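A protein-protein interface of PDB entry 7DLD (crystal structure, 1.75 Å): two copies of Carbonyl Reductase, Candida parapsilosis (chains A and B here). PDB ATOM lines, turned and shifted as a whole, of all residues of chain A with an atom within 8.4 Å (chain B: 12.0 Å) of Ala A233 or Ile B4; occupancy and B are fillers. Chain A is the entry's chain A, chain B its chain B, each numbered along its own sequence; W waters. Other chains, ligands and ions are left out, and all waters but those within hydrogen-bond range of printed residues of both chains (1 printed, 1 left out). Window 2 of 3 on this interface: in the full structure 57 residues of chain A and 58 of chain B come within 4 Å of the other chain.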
ATOM      1  N   ILE A 180      36.823  17.844  14.485  1.00  0.00           N
ATOM      2  CA  ILE A 180      36.102  17.499  15.711  1.00  0.00           C
ATOM      3  C   ILE A 180      35.320  16.217  15.472  1.00  0.00           C
ATOM      4  O   ILE A 180      34.885  15.941  14.351  1.00  0.00           O
ATOM      5  CB  ILE A 180      35.144  18.630  16.140  1.00  0.00           C
ATOM      6  CG1 ILE A 180      34.131  18.935  15.026  1.00  0.00           C
ATOM      7  CG2 ILE A 180      35.958  19.900  16.534  1.00  0.00           C
ATOM      8  CD1 ILE A 180      32.974  19.839  15.471  1.00  0.00           C
ATOM      9  N   PRO A 181      35.135  15.393  16.528  1.00  0.00           N
ATOM     10  CA  PRO A 181      35.548  15.533  17.930  1.00  0.00           C
ATOM     11  C   PRO A 181      36.954  15.037  18.237  1.00  0.00           C
ATOM     12  O   PRO A 181      37.377  15.144  19.385  1.00  0.00           O
ATOM     13  CB  PRO A 181      34.528  14.663  18.672  1.00  0.00           C
ATOM     14  CG  PRO A 181      34.281  13.531  17.717  1.00  0.00           C
ATOM     15  CD  PRO A 181      34.279  14.198  16.340  1.00  0.00           C
ATOM     16  N   ALA A 227      38.787   5.067  14.922  1.00  0.00           N
ATOM     17  CA  ALA A 227      37.602   5.892  14.721  1.00  0.00           C
ATOM     18  C   ALA A 227      36.377   5.090  15.138  1.00  0.00           C
ATOM     19  O   ALA A 227      35.971   4.156  14.438  1.00  0.00           O
ATOM     20  CB  ALA A 227      37.485   6.343  13.268  1.00  0.00           C
ATOM     21  N   SER A 228      35.789   5.459  16.273  1.00  0.00           N
ATOM     22  CA  SER A 228      34.579   4.803  16.741  1.00  0.00           C
ATOM     23  C   SER A 228      33.415   5.093  15.797  1.00  0.00           C
ATOM     24  O   SER A 228      33.474   5.982  14.936  1.00  0.00           O
ATOM     25  CB  SER A 228      34.231   5.269  18.149  1.00  0.00           C
ATOM     26  OG  SER A 228      34.017   6.672  18.167  1.00  0.00           O
ATOM     27  N   LYS A 229      32.339   4.322  15.974  1.00  0.00           N
ATOM     28  CA  LYS A 229      31.131   4.530  15.183  1.00  0.00           C
ATOM     29  C   LYS A 229      30.517   5.893  15.478  1.00  0.00           C
ATOM     30  O   LYS A 229      30.023   6.575  14.571  1.00  0.00           O
ATOM     31  CB  LYS A 229      30.119   3.415  15.469  1.00  0.00           C
ATOM     32  CG  LYS A 229      29.256   2.997  14.273  1.00  0.00           C
ATOM     33  CD  LYS A 229      28.295   4.095  13.818  1.00  0.00           C
ATOM     34  CE  LYS A 229      27.657   3.775  12.470  1.00  0.00           C
ATOM     35  NZ  LYS A 229      26.414   2.954  12.584  1.00  0.00           N
ATOM     36  N   ASP A 230      30.526   6.307  16.745  1.00  0.00           N
ATOM     37  CA  ASP A 230      29.927   7.591  17.068  1.00  0.00           C
ATOM     38  C   ASP A 230      30.779   8.754  16.587  1.00  0.00           C
ATOM     39  O   ASP A 230      30.242   9.829  16.326  1.00  0.00           O
ATOM     40  CB  ASP A 230      29.659   7.683  18.568  1.00  0.00           C
ATOM     41  CG  ASP A 230      28.556   6.735  19.007  1.00  0.00           C
ATOM     42  OD1 ASP A 230      28.647   6.184  20.119  1.00  0.00           O
ATOM     43  OD2 ASP A 230      27.611   6.520  18.216  1.00  0.00           O
ATOM     44  N   MET A 231      32.084   8.552  16.431  1.00  0.00           N
ATOM     45  CA  MET A 231      32.917   9.566  15.798  1.00  0.00           C
ATOM     46  C   MET A 231      32.569   9.725  14.320  1.00  0.00           C
ATOM     47  O   MET A 231      32.253  10.827  13.860  1.00  0.00           O
ATOM     48  CB  MET A 231      34.392   9.208  15.984  1.00  0.00           C
ATOM     49  CG  MET A 231      35.357  10.276  15.523  1.00  0.00           C
ATOM     50  SD  MET A 231      37.060   9.785  15.882  1.00  0.00           S
ATOM     51  CE  MET A 231      37.026   9.675  17.668  1.00  0.00           C
ATOM     52  N   LYS A 232      32.597   8.626  13.562  1.00  0.00           N
ATOM     53  CA  LYS A 232      32.245   8.704  12.147  1.00  0.00           C
ATOM     54  C   LYS A 232      30.838   9.259  11.965  1.00  0.00           C
ATOM     55  O   LYS A 232      30.562   9.993  11.007  1.00  0.00           O
ATOM     56  CB  LYS A 232      32.349   7.320  11.496  1.00  0.00           C
ATOM     57  CG  LYS A 232      33.756   6.788  11.253  1.00  0.00           C
ATOM     58  CD  LYS A 232      33.677   5.343  10.753  1.00  0.00           C
ATOM     59  CE  LYS A 232      35.040   4.777  10.378  1.00  0.00           C
ATOM     60  NZ  LYS A 232      35.411   5.058   8.960  1.00  0.00           N
ATOM     61  N   ALA A 233      29.925   8.899  12.868  1.00  0.00           N
ATOM     62  CA  ALA A 233      28.574   9.428  12.768  1.00  0.00           C
ATOM     63  C   ALA A 233      28.589  10.950  12.801  1.00  0.00           C
ATOM     64  O   ALA A 233      27.892  11.604  12.019  1.00  0.00           O
ATOM     65  CB  ALA A 233      27.699   8.874  13.889  1.00  0.00           C
ATOM     66  N   LYS A 234      29.394  11.528  13.682  1.00  0.00           N
ATOM     67  CA  LYS A 234      29.449  12.984  13.755  1.00  0.00           C
ATOM     68  C   LYS A 234      30.069  13.569  12.500  1.00  0.00           C
ATOM     69  O   LYS A 234      29.639  14.627  12.039  1.00  0.00           O
ATOM     70  CB  LYS A 234      30.216  13.420  15.006  1.00  0.00           C
ATOM     71  CG  LYS A 234      29.431  13.136  16.296  1.00  0.00           C
ATOM     72  CD  LYS A 234      30.231  13.570  17.515  1.00  0.00           C
ATOM     73  CE  LYS A 234      29.409  13.433  18.781  1.00  0.00           C
ATOM     74  NZ  LYS A 234      29.124  12.009  19.097  1.00  0.00           N
ATOM     75  N   TRP A 235      31.070  12.895  11.921  1.00  0.00           N
ATOM     76  CA  TRP A 235      31.604  13.364  10.651  1.00  0.00           C
ATOM     77  C   TRP A 235      30.519  13.386   9.583  1.00  0.00           C
ATOM     78  O   TRP A 235      30.405  14.352   8.832  1.00  0.00           O
ATOM     79  CB  TRP A 235      32.756  12.488  10.172  1.00  0.00           C
ATOM     80  CG  TRP A 235      33.930  12.366  11.041  1.00  0.00           C
ATOM     81  CD1 TRP A 235      34.273  13.154  12.104  1.00  0.00           C
ATOM     82  CD2 TRP A 235      34.944  11.358  10.935  1.00  0.00           C
ATOM     83  NE1 TRP A 235      35.443  12.686  12.666  1.00  0.00           N
ATOM     84  CE2 TRP A 235      35.873  11.589  11.966  1.00  0.00           C
ATOM     85  CE3 TRP A 235      35.160  10.289  10.057  1.00  0.00           C
ATOM     86  CZ2 TRP A 235      37.008  10.791  12.142  1.00  0.00           C
ATOM     87  CZ3 TRP A 235      36.271   9.477  10.252  1.00  0.00           C
ATOM     88  CH2 TRP A 235      37.186   9.740  11.276  1.00  0.00           C
ATOM     89  N   TRP A 236      29.720  12.316   9.488  1.00  0.00           N
ATOM     90  CA  TRP A 236      28.689  12.277   8.459  1.00  0.00           C
ATOM     91  C   TRP A 236      27.680  13.402   8.656  1.00  0.00           C
ATOM     92  O   TRP A 236      27.190  13.985   7.676  1.00  0.00           O
ATOM     93  CB  TRP A 236      27.935  10.938   8.481  1.00  0.00           C
ATOM     94  CG  TRP A 236      28.782   9.740   8.297  1.00  0.00           C
ATOM     95  CD1 TRP A 236      29.980   9.668   7.643  1.00  0.00           C
ATOM     96  CD2 TRP A 236      28.500   8.419   8.775  1.00  0.00           C
ATOM     97  NE1 TRP A 236      30.463   8.379   7.693  1.00  0.00           N
ATOM     98  CE2 TRP A 236      29.571   7.593   8.375  1.00  0.00           C
ATOM     99  CE3 TRP A 236      27.447   7.857   9.502  1.00  0.00           C
ATOM    100  CZ2 TRP A 236      29.619   6.232   8.683  1.00  0.00           C
ATOM    101  CZ3 TRP A 236      27.497   6.504   9.814  1.00  0.00           C
ATOM    102  CH2 TRP A 236      28.574   5.708   9.397  1.00  0.00           C
ATOM    103  N   GLN A 237      27.322  13.673   9.921  1.00  0.00           N
ATOM    104  CA  GLN A 237      26.323  14.690  10.246  1.00  0.00           C
ATOM    105  C   GLN A 237      26.776  16.084   9.844  1.00  0.00           C
ATOM    106  O   GLN A 237      25.940  16.939   9.553  1.00  0.00           O
ATOM    107  CB  GLN A 237      26.042  14.686  11.745  1.00  0.00           C
ATOM    108  CG  GLN A 237      25.158  13.535  12.229  1.00  0.00           C
ATOM    109  CD  GLN A 237      24.925  13.580  13.737  1.00  0.00           C
ATOM    110  OE1 GLN A 237      25.874  13.768  14.513  1.00  0.00           O
ATOM    111  NE2 GLN A 237      23.666  13.411  14.166  1.00  0.00           N
ATOM    112  N   LEU A 238      28.077  16.340   9.871  1.00  0.00           N
ATOM    113  CA  LEU A 238      28.634  17.646   9.522  1.00  0.00           C
ATOM    114  C   LEU A 238      29.076  17.749   8.063  1.00  0.00           C
ATOM    115  O   LEU A 238      29.549  18.817   7.638  1.00  0.00           O
ATOM    116  CB  LEU A 238      29.812  17.958  10.460  1.00  0.00           C
ATOM    117  CG  LEU A 238      29.372  18.004  11.926  1.00  0.00           C
ATOM    118  CD1 LEU A 238      30.555  18.183  12.891  1.00  0.00           C
ATOM    119  CD2 LEU A 238      28.350  19.103  12.133  1.00  0.00           C
ATOM    120  N   THR A 239      28.941  16.667   7.277  1.00  0.00           N
ATOM    121  CA  THR A 239      29.353  16.651   5.878  1.00  0.00           C
ATOM    122  C   THR A 239      28.141  16.895   5.002  1.00  0.00           C
ATOM    123  O   THR A 239      27.195  16.092   5.052  1.00  0.00           O
ATOM    124  CB  THR A 239      29.988  15.309   5.519  1.00  0.00           C
ATOM    125  OG1 THR A 239      31.113  15.079   6.365  1.00  0.00           O
ATOM    126  CG2 THR A 239      30.435  15.280   4.037  1.00  0.00           C
ATOM    127  N   GLY A 242      26.871  13.977   3.277  1.00  0.00           N
ATOM    128  CA  GLY A 242      26.292  13.018   4.207  1.00  0.00           C
ATOM    129  C   GLY A 242      27.027  11.705   4.347  1.00  0.00           C
ATOM    130  O   GLY A 242      26.449  10.742   4.855  1.00  0.00           O
ATOM    131  N   ARG A 243      28.285  11.640   3.932  1.00  0.00           N
ATOM    132  CA  ARG A 243      29.025  10.386   3.862  1.00  0.00           C
ATOM    133  C   ARG A 243      30.510  10.711   3.796  1.00  0.00           C
ATOM    134  O   ARG A 243      30.911  11.853   3.560  1.00  0.00           O
ATOM    135  CB  ARG A 243      28.607   9.557   2.631  1.00  0.00           C
ATOM    136  CG  ARG A 243      28.821  10.249   1.292  1.00  0.00           C
ATOM    137  CD  ARG A 243      28.546   9.297   0.112  1.00  0.00           C
ATOM    138  NE  ARG A 243      28.645   9.931  -1.208  1.00  0.00           N
ATOM    139  CZ  ARG A 243      29.773  10.051  -1.917  1.00  0.00           C
ATOM    140  NH1 ARG A 243      30.926   9.597  -1.442  1.00  0.00           N
ATOM    141  NH2 ARG A 243      29.752  10.648  -3.104  1.00  0.00           N
ATOM    142  N   GLU A 244      31.319   9.680   4.001  1.00  0.00           N
ATOM    143  CA  GLU A 244      32.726   9.717   3.644  1.00  0.00           C
ATOM    144  C   GLU A 244      32.903   9.519   2.141  1.00  0.00           C
ATOM    145  O   GLU A 244      32.059   8.925   1.473  1.00  0.00           O
ATOM    146  CB  GLU A 244      33.474   8.626   4.410  1.00  0.00           C
ATOM    147  CG  GLU A 244      33.498   8.832   5.908  1.00  0.00           C
ATOM    148  CD  GLU A 244      33.955   7.588   6.670  1.00  0.00           C
ATOM    149  OE1 GLU A 244      33.086   6.801   7.100  1.00  0.00           O
ATOM    150  OE2 GLU A 244      35.182   7.396   6.836  1.00  0.00           O
ATOM    151  N   MET B   1      14.347   8.818  15.462  1.00  0.00           N
ATOM    152  CA  MET B   1      14.795   7.864  16.482  1.00  0.00           C
ATOM    153  C   MET B   1      15.345   6.624  15.775  1.00  0.00           C
ATOM    154  O   MET B   1      14.694   6.048  14.902  1.00  0.00           O
ATOM    155  CB  MET B   1      13.656   7.498  17.448  1.00  0.00           C
ATOM    156  CG  MET B   1      14.109   6.833  18.730  1.00  0.00           C
ATOM    157  SD  MET B   1      12.862   6.609  20.054  1.00  0.00           S
ATOM    158  CE  MET B   1      13.861   5.762  21.271  1.00  0.00           C
ATOM    159  N   GLY B   2      16.568   6.239  16.122  1.00  0.00           N
ATOM    160  CA  GLY B   2      17.242   5.161  15.449  1.00  0.00           C
ATOM    161  C   GLY B   2      18.079   5.573  14.252  1.00  0.00           C
ATOM    162  O   GLY B   2      19.083   4.921  13.968  1.00  0.00           O
ATOM    163  N   GLU B   3      17.687   6.618  13.531  1.00  0.00           N
ATOM    164  CA  GLU B   3      18.473   7.088  12.396  1.00  0.00           C
ATOM    165  C   GLU B   3      19.507   8.110  12.842  1.00  0.00           C
ATOM    166  O   GLU B   3      19.335   8.799  13.855  1.00  0.00           O
ATOM    167  CB  GLU B   3      17.573   7.711  11.332  1.00  0.00           C
ATOM    168  CG  GLU B   3      16.418   6.829  10.918  1.00  0.00           C
ATOM    169  CD  GLU B   3      15.273   7.622  10.331  1.00  0.00           C
ATOM    170  OE1 GLU B   3      14.414   7.009   9.656  1.00  0.00           O
ATOM    171  OE2 GLU B   3      15.231   8.854  10.551  1.00  0.00           O
ATOM    172  N   ILE B   4      20.592   8.193  12.078  1.00  0.00           N
ATOM    173  CA  ILE B   4      21.530   9.302  12.180  1.00  0.00           C
ATOM    174  C   ILE B   4      21.037  10.401  11.255  1.00  0.00           C
ATOM    175  O   ILE B   4      21.010  10.225  10.030  1.00  0.00           O
ATOM    176  CB  ILE B   4      22.950   8.882  11.797  1.00  0.00           C
ATOM    177  CG1 ILE B   4      23.485   7.825  12.749  1.00  0.00           C
ATOM    178  CG2 ILE B   4      23.861  10.108  11.800  1.00  0.00           C
ATOM    179  CD1 ILE B   4      24.762   7.168  12.260  1.00  0.00           C
ATOM    180  N   GLU B   5      20.658  11.536  11.833  1.00  0.00           N
ATOM    181  CA  GLU B   5      20.077  12.633  11.073  1.00  0.00           C
ATOM    182  C   GLU B   5      21.131  13.704  10.867  1.00  0.00           C
ATOM    183  O   GLU B   5      21.855  14.046  11.806  1.00  0.00           O
ATOM    184  CB  GLU B   5      18.847  13.204  11.783  1.00  0.00           C
ATOM    185  CG  GLU B   5      17.615  12.309  11.618  1.00  0.00           C
ATOM    186  CD  GLU B   5      16.501  12.622  12.597  1.00  0.00           C
ATOM    187  OE1 GLU B   5      16.737  13.394  13.551  1.00  0.00           O
ATOM    188  OE2 GLU B   5      15.386  12.085  12.416  1.00  0.00           O
ATOM    189  N   SER B   6      21.228  14.196   9.634  1.00  0.00           N
ATOM    190  CA  SER B   6      22.223  15.208   9.287  1.00  0.00           C
ATOM    191  C   SER B   6      22.016  16.485  10.089  1.00  0.00           C
ATOM    192  O   SER B   6      20.883  16.914  10.328  1.00  0.00           O
ATOM    193  CB  SER B   6      22.133  15.522   7.799  1.00  0.00           C
ATOM    194  OG  SER B   6      22.940  16.637   7.422  1.00  0.00           O
ATOM    195  N   TYR B   7      23.122  17.110  10.486  1.00  0.00           N
ATOM    196  CA  TYR B   7      23.052  18.480  10.969  1.00  0.00           C
ATOM    197  C   TYR B   7      22.991  19.484   9.823  1.00  0.00           C
ATOM    198  O   TYR B   7      22.557  20.616  10.039  1.00  0.00           O
ATOM    199  CB  TYR B   7      24.243  18.804  11.876  1.00  0.00           C
ATOM    200  CG  TYR B   7      24.087  18.372  13.326  1.00  0.00           C
ATOM    201  CD1 TYR B   7      24.668  19.116  14.359  1.00  0.00           C
ATOM    202  CD2 TYR B   7      23.382  17.217  13.679  1.00  0.00           C
ATOM    203  CE1 TYR B   7      24.540  18.740  15.685  1.00  0.00           C
ATOM    204  CE2 TYR B   7      23.243  16.840  14.981  1.00  0.00           C
ATOM    205  CZ  TYR B   7      23.822  17.595  15.991  1.00  0.00           C
ATOM    206  OH  TYR B   7      23.676  17.210  17.288  1.00  0.00           O
ATOM    207  N   CYS B   8      23.419  19.102   8.612  1.00  0.00           N
ATOM    208  CA  CYS B   8      23.354  20.013   7.469  1.00  0.00           C
ATOM    209  C   CYS B   8      21.967  20.057   6.826  1.00  0.00           C
ATOM    210  O   CYS B   8      21.445  21.141   6.536  1.00  0.00           O
ATOM    211  CB  CYS B   8      24.389  19.608   6.419  1.00  0.00           C
ATOM    212  SG  CYS B   8      26.068  19.611   7.046  1.00  0.00           S
ATOM    213  N   ASN B   9      21.372  18.897   6.542  1.00  0.00           N
ATOM    214  CA  ASN B   9      20.164  18.871   5.717  1.00  0.00           C
ATOM    215  C   ASN B   9      19.437  17.549   5.945  1.00  0.00           C
ATOM    216  O   ASN B   9      19.856  16.515   5.408  1.00  0.00           O
ATOM    217  CB  ASN B   9      20.522  19.050   4.247  1.00  0.00           C
ATOM    218  CG  ASN B   9      19.308  19.323   3.377  1.00  0.00           C
ATOM    219  OD1 ASN B   9      18.179  19.069   3.780  1.00  0.00           O
ATOM    220  ND2 ASN B   9      19.544  19.856   2.176  1.00  0.00           N
ATOM    221  N   LYS B  10      18.328  17.598   6.683  1.00  0.00           N
ATOM    222  CA  LYS B  10      17.586  16.381   6.992  1.00  0.00           C
ATOM    223  C   LYS B  10      17.026  15.715   5.744  1.00  0.00           C
ATOM    224  O   LYS B  10      16.591  14.558   5.825  1.00  0.00           O
ATOM    225  CB  LYS B  10      16.435  16.672   7.965  1.00  0.00           C
ATOM    226  CG  LYS B  10      16.642  17.881   8.866  1.00  0.00           C
ATOM    227  CD  LYS B  10      17.813  17.692   9.817  1.00  0.00           C
ATOM    228  CE  LYS B  10      18.313  19.037  10.332  1.00  0.00           C
ATOM    229  NZ  LYS B  10      19.562  18.919  11.128  1.00  0.00           N
ATOM    230  N   GLU B  11      17.013  16.408   4.602  1.00  0.00           N
ATOM    231  CA  GLU B  11      16.514  15.802   3.371  1.00  0.00           C
ATOM    232  C   GLU B  11      17.479  14.771   2.817  1.00  0.00           C
ATOM    233  O   GLU B  11      17.138  14.075   1.857  1.00  0.00           O
ATOM    234  CB  GLU B  11      16.216  16.876   2.328  1.00  0.00           C
ATOM    235  CG  GLU B  11      15.057  17.777   2.693  1.00  0.00           C
ATOM    236  CD  GLU B  11      13.715  17.131   2.425  1.00  0.00           C
ATOM    237  OE1 GLU B  11      13.453  16.780   1.254  1.00  0.00           O
ATOM    238  OE2 GLU B  11      12.930  16.968   3.386  1.00  0.00           O
ATOM    239  N   LEU B  12      18.680  14.662   3.393  1.00  0.00           N
ATOM    240  CA  LEU B  12      19.597  13.588   3.031  1.00  0.00           C
ATOM    241  C   LEU B  12      19.068  12.216   3.427  1.00  0.00           C
ATOM    242  O   LEU B  12      19.481  11.210   2.836  1.00  0.00           O
ATOM    243  CB  LEU B  12      20.954  13.816   3.697  1.00  0.00           C
ATOM    244  CG  LEU B  12      21.710  15.023   3.128  1.00  0.00           C
ATOM    245  CD1 LEU B  12      22.859  15.426   4.065  1.00  0.00           C
ATOM    246  CD2 LEU B  12      22.247  14.725   1.716  1.00  0.00           C
ATOM    247  N   GLY B  13      18.166  12.159   4.400  1.00  0.00           N
ATOM    248  CA  GLY B  13      17.700  10.902   4.942  1.00  0.00           C
ATOM    249  C   GLY B  13      18.688  10.314   5.932  1.00  0.00           C
ATOM    250  O   GLY B  13      19.693  10.940   6.287  1.00  0.00           O
ATOM    251  N   PRO B  14      18.423   9.093   6.398  1.00  0.00           N
ATOM    252  CA  PRO B  14      19.301   8.470   7.397  1.00  0.00           C
ATOM    253  C   PRO B  14      20.721   8.316   6.885  1.00  0.00           C
ATOM    254  O   PRO B  14      20.950   7.865   5.763  1.00  0.00           O
ATOM    255  CB  PRO B  14      18.640   7.109   7.640  1.00  0.00           C
ATOM    256  CG  PRO B  14      17.226   7.320   7.272  1.00  0.00           C
ATOM    257  CD  PRO B  14      17.237   8.260   6.123  1.00  0.00           C
ATOM    258  N   LEU B  15      21.707   8.697   7.755  1.00  0.00           N
ATOM    259  CA  LEU B  15      23.088   8.705   7.302  1.00  0.00           C
ATOM    260  C   LEU B  15      23.761   7.369   7.605  1.00  0.00           C
ATOM    261  O   LEU B  15      23.355   6.661   8.528  1.00  0.00           O
ATOM    262  CB  LEU B  15      23.858   9.831   7.985  1.00  0.00           C
ATOM    263  CG  LEU B  15      23.340  11.231   7.682  1.00  0.00           C
ATOM    264  CD1 LEU B  15      24.241  12.279   8.419  1.00  0.00           C
ATOM    265  CD2 LEU B  15      23.270  11.483   6.182  1.00  0.00           C
ATOM    266  N   PRO B  16      24.812   7.009   6.844  1.00  0.00           N
ATOM    267  CA  PRO B  16      25.418   7.785   5.748  1.00  0.00           C
ATOM    268  C   PRO B  16      24.678   7.599   4.441  1.00  0.00           C
ATOM    269  O   PRO B  16      24.070   6.531   4.231  1.00  0.00           O
ATOM    270  CB  PRO B  16      26.826   7.199   5.635  1.00  0.00           C
ATOM    271  CG  PRO B  16      26.635   5.764   6.047  1.00  0.00           C
ATOM    272  CD  PRO B  16      25.579   5.786   7.142  1.00  0.00           C
ATOM    273  N   THR B  17      24.682   8.631   3.607  1.00  0.00           N
ATOM    274  CA  THR B  17      24.246   8.461   2.233  1.00  0.00           C
ATOM    275  C   THR B  17      25.213   7.533   1.514  1.00  0.00           C
ATOM    276  O   THR B  17      26.273   7.167   2.036  1.00  0.00           O
ATOM    277  CB  THR B  17      24.175   9.803   1.514  1.00  0.00           C
ATOM    278  OG1 THR B  17      25.488  10.386   1.475  1.00  0.00           O
ATOM    279  CG2 THR B  17      23.198  10.730   2.243  1.00  0.00           C
ATOM    280  N   LYS B  18      24.855   7.166   0.293  1.00  0.00           N
ATOM    281  CA  LYS B  18      25.601   6.151  -0.427  1.00  0.00           C
ATOM    282  C   LYS B  18      26.302   6.738  -1.647  1.00  0.00           C
ATOM    283  O   LYS B  18      25.801   7.654  -2.306  1.00  0.00           O
ATOM    284  CB  LYS B  18      24.675   4.995  -0.818  1.00  0.00           C
ATOM    285  CG  LYS B  18      24.058   4.320   0.403  1.00  0.00           C
ATOM    286  CD  LYS B  18      25.131   3.860   1.398  1.00  0.00           C
ATOM    287  CE  LYS B  18      24.563   2.965   2.503  1.00  0.00           C
ATOM    288  NZ  LYS B  18      23.683   3.690   3.458  1.00  0.00           N
ATOM    289  N   PRO B 207      21.149  16.589  -1.322  1.00  0.00           N
ATOM    290  CA  PRO B 207      20.474  15.310  -1.575  1.00  0.00           C
ATOM    291  C   PRO B 207      20.300  15.011  -3.044  1.00  0.00           C
ATOM    292  O   PRO B 207      20.010  13.860  -3.385  1.00  0.00           O
ATOM    293  CB  PRO B 207      19.107  15.477  -0.880  1.00  0.00           C
ATOM    294  CG  PRO B 207      19.344  16.546   0.129  1.00  0.00           C
ATOM    295  CD  PRO B 207      20.280  17.484  -0.539  1.00  0.00           C
HETATM  296  O   HOH W   1      20.654  11.808  14.733  1.00  0.00           O
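N of Thr B17 sits at hydrogen-bond distance from O of Gly A242, at 3.0 Å.
O of Gln A237 lies within hydrogen-bond range of N of Cys B8 (3.5 Å).
The side-chain sulfur (SG) of Cys B8 is in hydrogen-bond range of the backbone carbonyl oxygen (O) of Leu A238 (3.6 Å).
NE2 of Gln A237 is in hydrogen-bond range of O of Glu B5 (3.0 Å).
The backbone NH (N) of Tyr B7 is in hydrogen-bond range of the backbone carbonyl oxygen (O) of Gln A237, 3.0 Å away.
The side-chain hydroxyl (OG) of Ser B6 is in hydrogen-bond range of the backbone NH (N) of Asn B9 (2.9 Å).
N of Cys B8 sits at hydrogen-bond distance from OG of Ser B6, 2.8 Å away.
The backbone carbonyl oxygen (O) of Ser B6 sits at hydrogen-bond distance from the side-chain amino group (NZ) of Lys B10, at 2.5 Å.
The backbone carbonyl oxygen (O) of Trp A235 is in hydrogen-bond range of the side-chain hydroxyl (OG1) of Thr A239 (2.7 Å).
The backbone carbonyl oxygen (O) of Pro B16 lies within hydrogen-bond range of the side-chain amino group (NZ) of Lys B18 (3.0 Å).
O of Ile B4 lies within hydrogen-bond range of N of Leu B15 (2.8 Å).
Among the printed residues, merely in contact across the chains: Ala A233 with Ile B4 (3.8 Å), Trp A236 with Ile B4 (3.7 Å), Trp A236 with Leu B15 (3.5 Å), Trp A236 with Pro B16 (3.4 Å), Gln A237 with Ile B4 (3.7 Å), Gln A237 with Ser B6 (3.7 Å), Gln A237 with Leu B15 (3.7 Å), Thr A239 with Cys B8 (3.98 Å), Gly A242 with Leu B15 (3.5 Å), Gly A242 with Pro B16 (3.3 Å), Arg A243 with Thr B17 (3.3 Å) and Arg A243 with Lys B18 (3.8 Å).
No residue of chain B comes within 4 Å of Ser A228.
Ala A233 touches just one residue of chain B: Ile B4.
Lys A234 touches none of the printed residues of chain B.
No residue of chain B comes within 4 Å of Trp A235.
Trp A236 touches three residues of chain B.
Of chain B, only Ile B4 (3.7 Å), Glu B5 (3.0 Å), Ser B6 (3.7 Å), Tyr B7 (3.0 Å), Cys B8 (3.5 Å) and Leu B15 (3.7 Å) come within 4 Å of Gln A237.
Of the printed residues of chain B, Leu A238 touches Cys B8.
Printed residues of chain B within 4 Å of Gly A242: Leu B15, Pro B16 and Thr B17.
Of the printed residues of chain A, Ile B4 touches Ala A233, Trp A236 and Gln A237.
Printed residues of chain A within 4 Å of Tyr B7: Gln A237.
Printed residues of chain A within 4 Å of Cys B8: Gln A237 (3.5 Å), Leu A238 (3.6 Å) and Thr A239 (3.98 Å).
Pro B14 touches none of the printed residues of chain A.
Of the printed residues of chain A, Pro B16 touches Trp A236 (3.4 Å) and Gly A242 (3.3 Å).
The nearest residue of chain A that does not touch Ile B4 is Lys A229 (4.5 Å).
Printed residues of chain B that touch a printed residue of chain A: Ile B4, Glu B5, Ser B6, Tyr B7, Cys B8, Leu B15, Pro B16, Thr B17 and Lys B18.
Hydrophobic or aromatic side chains of chain B that line the printed part of chain A: Ile B4, Tyr B7, Leu B15 and Pro B16.
Among the printed residues, 17 pairs touch across the chains.
Among the printed residues, no Asp or Glu carboxylate lies within 4 Å of a Lys or Arg side-chain nitrogen of the other chain.
No position is printed for both chains.
Of the 17 pairs that touch across the chains among the printed residues, none has its exchanged pair printed and touching as well.
Water W1 lies within hydrogen-bond range of N of Glu B5 (2.9 Å), O of Glu B3 (3.4 Å) and NE2 of Gln A237 (3.5 Å).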
